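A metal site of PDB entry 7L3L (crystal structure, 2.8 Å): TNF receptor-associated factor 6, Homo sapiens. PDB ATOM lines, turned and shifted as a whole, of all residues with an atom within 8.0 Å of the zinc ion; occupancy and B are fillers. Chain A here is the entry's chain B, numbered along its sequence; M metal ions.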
ATOM      1  N   LYS A  82     -17.436  -3.661  -0.473  1.00  0.00           N
ATOM      2  CA  LYS A  82     -16.820  -3.897  -1.778  1.00  0.00           C
ATOM      3  C   LYS A  82     -15.667  -4.871  -1.609  1.00  0.00           C
ATOM      4  O   LYS A  82     -14.967  -4.862  -0.602  1.00  0.00           O
ATOM      5  CB  LYS A  82     -16.323  -2.576  -2.395  1.00  0.00           C
ATOM      6  CG  LYS A  82     -17.363  -1.464  -2.407  1.00  0.00           C
ATOM      7  CD  LYS A  82     -16.759  -0.139  -2.855  1.00  0.00           C
ATOM      8  CE  LYS A  82     -16.501  -0.106  -4.363  1.00  0.00           C
ATOM      9  NZ  LYS A  82     -16.225   1.281  -4.852  1.00  0.00           N
ATOM     10  N   CYS A  83     -15.482  -5.727  -2.609  1.00  0.00           N
ATOM     11  CA  CYS A  83     -14.345  -6.637  -2.621  1.00  0.00           C
ATOM     12  C   CYS A  83     -13.099  -5.855  -3.009  1.00  0.00           C
ATOM     13  O   CYS A  83     -13.058  -5.288  -4.111  1.00  0.00           O
ATOM     14  CB  CYS A  83     -14.572  -7.783  -3.584  1.00  0.00           C
ATOM     15  SG  CYS A  83     -13.110  -8.790  -3.924  1.00  0.00           S
ATOM     16  N   PRO A  84     -12.053  -5.817  -2.177  1.00  0.00           N
ATOM     17  CA  PRO A  84     -10.961  -4.860  -2.390  1.00  0.00           C
ATOM     18  C   PRO A  84     -10.083  -5.169  -3.595  1.00  0.00           C
ATOM     19  O   PRO A  84      -9.169  -4.384  -3.873  1.00  0.00           O
ATOM     20  CB  PRO A  84     -10.160  -4.963  -1.089  1.00  0.00           C
ATOM     21  CG  PRO A  84     -10.369  -6.368  -0.643  1.00  0.00           C
ATOM     22  CD  PRO A  84     -11.789  -6.707  -1.034  1.00  0.00           C
ATOM     23  N   ASN A  85     -10.328  -6.268  -4.307  1.00  0.00           N
ATOM     24  CA  ASN A  85      -9.457  -6.666  -5.403  1.00  0.00           C
ATOM     25  C   ASN A  85      -9.442  -5.608  -6.505  1.00  0.00           C
ATOM     26  O   ASN A  85     -10.416  -4.896  -6.729  1.00  0.00           O
ATOM     27  CB  ASN A  85      -9.908  -8.008  -5.960  1.00  0.00           C
ATOM     28  CG  ASN A  85      -9.588  -9.167  -5.034  1.00  0.00           C
ATOM     29  OD1 ASN A  85      -8.663  -9.087  -4.230  1.00  0.00           O
ATOM     30  ND2 ASN A  85     -10.353 -10.242  -5.139  1.00  0.00           N
ATOM     31  N   GLU A  86      -8.304  -5.528  -7.195  1.00  0.00           N
ATOM     32  CA  GLU A  86      -8.111  -4.522  -8.236  1.00  0.00           C
ATOM     33  C   GLU A  86      -9.020  -4.813  -9.433  1.00  0.00           C
ATOM     34  O   GLU A  86      -8.903  -5.877 -10.059  1.00  0.00           O
ATOM     35  CB  GLU A  86      -6.652  -4.489  -8.675  1.00  0.00           C
ATOM     36  CG  GLU A  86      -5.723  -3.766  -7.705  1.00  0.00           C
ATOM     37  CD  GLU A  86      -5.567  -2.293  -8.042  1.00  0.00           C
ATOM     38  OE1 GLU A  86      -6.417  -1.756  -8.786  1.00  0.00           O
ATOM     39  OE2 GLU A  86      -4.598  -1.675  -7.556  1.00  0.00           O
ATOM     40  N   GLY A  87      -9.908  -3.873  -9.743  1.00  0.00           N
ATOM     41  CA  GLY A  87     -10.753  -3.979 -10.918  1.00  0.00           C
ATOM     42  C   GLY A  87     -12.085  -4.678 -10.708  1.00  0.00           C
ATOM     43  O   GLY A  87     -12.892  -4.714 -11.639  1.00  0.00           O
ATOM     44  N   CYS A  88     -12.338  -5.227  -9.524  1.00  0.00           N
ATOM     45  CA  CYS A  88     -13.598  -5.905  -9.264  1.00  0.00           C
ATOM     46  C   CYS A  88     -14.585  -4.926  -8.635  1.00  0.00           C
ATOM     47  O   CYS A  88     -14.251  -4.239  -7.665  1.00  0.00           O
ATOM     48  CB  CYS A  88     -13.393  -7.112  -8.339  1.00  0.00           C
ATOM     49  SG  CYS A  88     -14.916  -7.998  -7.973  1.00  0.00           S
ATOM     50  N   LEU A  89     -15.796  -4.895  -9.186  1.00  0.00           N
ATOM     51  CA  LEU A  89     -16.851  -3.991  -8.727  1.00  0.00           C
ATOM     52  C   LEU A  89     -17.950  -4.744  -7.984  1.00  0.00           C
ATOM     53  O   LEU A  89     -19.093  -4.308  -7.951  1.00  0.00           O
ATOM     54  CB  LEU A  89     -17.436  -3.211  -9.894  1.00  0.00           C
ATOM     55  CG  LEU A  89     -16.454  -2.524 -10.852  1.00  0.00           C
ATOM     56  CD1 LEU A  89     -16.152  -3.414 -12.054  1.00  0.00           C
ATOM     57  CD2 LEU A  89     -16.982  -1.174 -11.292  1.00  0.00           C
ATOM     58  N   HIS A  90     -17.601  -5.875  -7.376  1.00  0.00           N
ATOM     59  CA  HIS A  90     -18.604  -6.699  -6.692  1.00  0.00           C
ATOM     60  C   HIS A  90     -18.861  -6.162  -5.298  1.00  0.00           C
ATOM     61  O   HIS A  90     -17.949  -6.102  -4.461  1.00  0.00           O
ATOM     62  CB  HIS A  90     -18.147  -8.149  -6.630  1.00  0.00           C
ATOM     63  CG  HIS A  90     -18.702  -9.002  -7.738  1.00  0.00           C
ATOM     64  ND1 HIS A  90     -17.897  -9.610  -8.670  1.00  0.00           N
ATOM     65  CD2 HIS A  90     -19.978  -9.326  -8.054  1.00  0.00           C
ATOM     66  CE1 HIS A  90     -18.655 -10.283  -9.525  1.00  0.00           C
ATOM     67  NE2 HIS A  90     -19.920 -10.123  -9.167  1.00  0.00           N
ATOM     68  N   LYS A  91     -20.106  -5.773  -5.039  1.00  0.00           N
ATOM     69  CA  LYS A  91     -20.566  -5.445  -3.707  1.00  0.00           C
ATOM     70  C   LYS A  91     -21.363  -6.618  -3.172  1.00  0.00           C
ATOM     71  O   LYS A  91     -22.229  -7.156  -3.867  1.00  0.00           O
ATOM     72  CB  LYS A  91     -21.425  -4.169  -3.719  1.00  0.00           C
ATOM     73  CG  LYS A  91     -20.740  -2.968  -4.351  1.00  0.00           C
ATOM     74  CD  LYS A  91     -21.737  -1.877  -4.738  1.00  0.00           C
ATOM     75  CE  LYS A  91     -21.042  -0.537  -4.954  1.00  0.00           C
ATOM     76  NZ  LYS A  91     -21.831   0.590  -4.364  1.00  0.00           N
ATOM     77  N   MET A  92     -21.061  -7.030  -1.943  1.00  0.00           N
ATOM     78  CA  MET A  92     -21.802  -8.085  -1.267  1.00  0.00           C
ATOM     79  C   MET A  92     -21.938  -7.732   0.202  1.00  0.00           C
ATOM     80  O   MET A  92     -21.285  -6.815   0.706  1.00  0.00           O
ATOM     81  CB  MET A  92     -21.141  -9.459  -1.437  1.00  0.00           C
ATOM     82  CG  MET A  92     -19.795  -9.599  -0.777  1.00  0.00           C
ATOM     83  SD  MET A  92     -18.479  -8.969  -1.813  1.00  0.00           S
ATOM     84  CE  MET A  92     -18.698  -9.987  -3.269  1.00  0.00           C
ATOM     85  N   LEU A  97     -18.275 -11.992   2.014  1.00  0.00           N
ATOM     86  CA  LEU A  97     -17.091 -11.453   1.366  1.00  0.00           C
ATOM     87  C   LEU A  97     -16.065 -12.541   1.076  1.00  0.00           C
ATOM     88  O   LEU A  97     -15.495 -12.580  -0.025  1.00  0.00           O
ATOM     89  CB  LEU A  97     -16.494 -10.337   2.216  1.00  0.00           C
ATOM     90  CG  LEU A  97     -15.315  -9.495   1.717  1.00  0.00           C
ATOM     91  CD1 LEU A  97     -13.997 -10.116   2.149  1.00  0.00           C
ATOM     92  CD2 LEU A  97     -15.336  -9.297   0.205  1.00  0.00           C
ATOM     93  N   HIS A 100     -17.140 -14.714  -1.845  1.00  0.00           N
ATOM     94  CA  HIS A 100     -16.876 -14.169  -3.170  1.00  0.00           C
ATOM     95  C   HIS A 100     -15.392 -14.220  -3.515  1.00  0.00           C
ATOM     96  O   HIS A 100     -15.029 -14.575  -4.642  1.00  0.00           O
ATOM     97  CB  HIS A 100     -17.396 -12.734  -3.261  1.00  0.00           C
ATOM     98  CG  HIS A 100     -16.799 -11.962  -4.407  1.00  0.00           C
ATOM     99  ND1 HIS A 100     -17.308 -12.032  -5.681  1.00  0.00           N
ATOM    100  CD2 HIS A 100     -15.742 -11.126  -4.463  1.00  0.00           C
ATOM    101  CE1 HIS A 100     -16.586 -11.261  -6.478  1.00  0.00           C
ATOM    102  NE2 HIS A 100     -15.623 -10.692  -5.760  1.00  0.00           N
ATOM    103  N   GLN A 101     -14.526 -13.845  -2.570  1.00  0.00           N
ATOM    104  CA  GLN A 101     -13.095 -13.796  -2.846  1.00  0.00           C
ATOM    105  C   GLN A 101     -12.539 -15.164  -3.215  1.00  0.00           C
ATOM    106  O   GLN A 101     -11.543 -15.256  -3.948  1.00  0.00           O
ATOM    107  CB  GLN A 101     -12.341 -13.229  -1.644  1.00  0.00           C
ATOM    108  CG  GLN A 101     -12.584 -11.743  -1.387  1.00  0.00           C
ATOM    109  CD  GLN A 101     -11.709 -11.213  -0.263  1.00  0.00           C
ATOM    110  OE1 GLN A 101     -11.674 -11.767   0.827  1.00  0.00           O
ATOM    111  NE2 GLN A 101     -11.000 -10.121  -0.532  1.00  0.00           N
ATOM    112  N   ALA A 102     -13.158 -16.239  -2.715  1.00  0.00           N
ATOM    113  CA  ALA A 102     -12.653 -17.585  -2.990  1.00  0.00           C
ATOM    114  C   ALA A 102     -12.649 -17.882  -4.478  1.00  0.00           C
ATOM    115  O   ALA A 102     -11.777 -18.612  -4.965  1.00  0.00           O
ATOM    116  CB  ALA A 102     -13.481 -18.616  -2.242  1.00  0.00           C
ATOM    117  N   HIS A 103     -13.603 -17.323  -5.224  1.00  0.00           N
ATOM    118  CA  HIS A 103     -13.669 -17.500  -6.668  1.00  0.00           C
ATOM    119  C   HIS A 103     -13.833 -16.156  -7.355  1.00  0.00           C
ATOM    120  O   HIS A 103     -14.554 -16.029  -8.348  1.00  0.00           O
ATOM    121  CB  HIS A 103     -14.789 -18.451  -7.058  1.00  0.00           C
ATOM    122  CG  HIS A 103     -14.760 -19.754  -6.334  1.00  0.00           C
ATOM    123  ND1 HIS A 103     -15.158 -19.886  -5.023  1.00  0.00           N
ATOM    124  CD2 HIS A 103     -14.398 -20.990  -6.748  1.00  0.00           C
ATOM    125  CE1 HIS A 103     -15.025 -21.151  -4.647  1.00  0.00           C
ATOM    126  NE2 HIS A 103     -14.565 -21.844  -5.682  1.00  0.00           N
ATOM    127  N   CYS A 104     -13.192 -15.120  -6.823  1.00  0.00           N
ATOM    128  CA  CYS A 104     -13.204 -13.816  -7.472  1.00  0.00           C
ATOM    129  C   CYS A 104     -12.254 -13.820  -8.663  1.00  0.00           C
ATOM    130  O   CYS A 104     -11.193 -14.463  -8.632  1.00  0.00           O
ATOM    131  CB  CYS A 104     -12.820 -12.713  -6.500  1.00  0.00           C
ATOM    132  SG  CYS A 104     -12.957 -11.069  -7.216  1.00  0.00           S
ATOM    133  N   GLU A 105     -12.640 -13.100  -9.716  1.00  0.00           N
ATOM    134  CA  GLU A 105     -11.893 -13.149 -10.968  1.00  0.00           C
ATOM    135  C   GLU A 105     -10.530 -12.476 -10.817  1.00  0.00           C
ATOM    136  O   GLU A 105      -9.507 -13.027 -11.239  1.00  0.00           O
ATOM    137  CB  GLU A 105     -12.699 -12.491 -12.075  1.00  0.00           C
ATOM    138  CG  GLU A 105     -14.004 -13.207 -12.381  1.00  0.00           C
ATOM    139  CD  GLU A 105     -13.848 -14.247 -13.465  1.00  0.00           C
ATOM    140  OE1 GLU A 105     -12.952 -14.068 -14.326  1.00  0.00           O
ATOM    141  OE2 GLU A 105     -14.603 -15.241 -13.450  1.00  0.00           O
ATOM    142  N   PHE A 106     -10.501 -11.294 -10.227  1.00  0.00           N
ATOM    143  CA  PHE A 106      -9.275 -10.497 -10.129  1.00  0.00           C
ATOM    144  C   PHE A 106      -8.590 -10.799  -8.792  1.00  0.00           C
ATOM    145  O   PHE A 106      -9.035 -10.330  -7.744  1.00  0.00           O
ATOM    146  CB  PHE A 106      -9.593  -9.011 -10.266  1.00  0.00           C
ATOM    147  CG  PHE A 106     -10.548  -8.703 -11.392  1.00  0.00           C
ATOM    148  CD1 PHE A 106     -10.276  -9.109 -12.685  1.00  0.00           C
ATOM    149  CD2 PHE A 106     -11.723  -8.015 -11.152  1.00  0.00           C
ATOM    150  CE1 PHE A 106     -11.155  -8.825 -13.718  1.00  0.00           C
ATOM    151  CE2 PHE A 106     -12.609  -7.731 -12.173  1.00  0.00           C
ATOM    152  CZ  PHE A 106     -12.328  -8.134 -13.462  1.00  0.00           C
ATOM    153  N   ALA A 107      -7.515 -11.577  -8.845  1.00  0.00           N
ATOM    154  CA  ALA A 107      -6.767 -11.903  -7.643  1.00  0.00           C
ATOM    155  C   ALA A 107      -5.324 -12.253  -7.976  1.00  0.00           C
ATOM    156  O   ALA A 107      -4.963 -12.414  -9.141  1.00  0.00           O
ATOM    157  CB  ALA A 107      -7.438 -13.060  -6.896  1.00  0.00           C
HETATM  158 ZN    ZN M   1     -13.974  -9.259  -6.192  1.00  0.00          ZN
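N of Cys 83 sits at hydrogen-bond distance from O of His 90, 3.1 Å away. The side-chain amide nitrogen (ND2) of Asn 85 lies within hydrogen-bond range of the backbone carbonyl oxygen (O) of Phe 106, at 2.9 Å. SG of Cys 104 sits close to ND2 of Asn 85, 3.4 Å away. The side-chain sulfur (SG) of Cys 88 sits close to a ring nitrogen (ND1) of His 90. ND2 of Asn 85 sits close to SG of Cys 83 (3.3 Å).
Merely in contact with the zinc ion: Asn 85 (3.9 Å). Five residues have an atom within 4 Å of the zinc ion: Cys 83, Asn 85, Cys 88, His 100 and Cys 104. The nearest printed residue that does not touch the zinc ion is His 90 (4.3 Å).
A ring nitrogen (NE2) of His 100 is bound to the zinc ion, at 2.2 Å. The zinc ion is bound by the side-chain sulfur (SG) of Cys 104 (2.3 Å). The zinc ion is bound by the side-chain sulfur (SG) of Cys 88 (2.4 Å). The side-chain sulfur (SG) of Cys 83 binds the zinc ion. The zinc ion has four donor atoms within binding distance.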
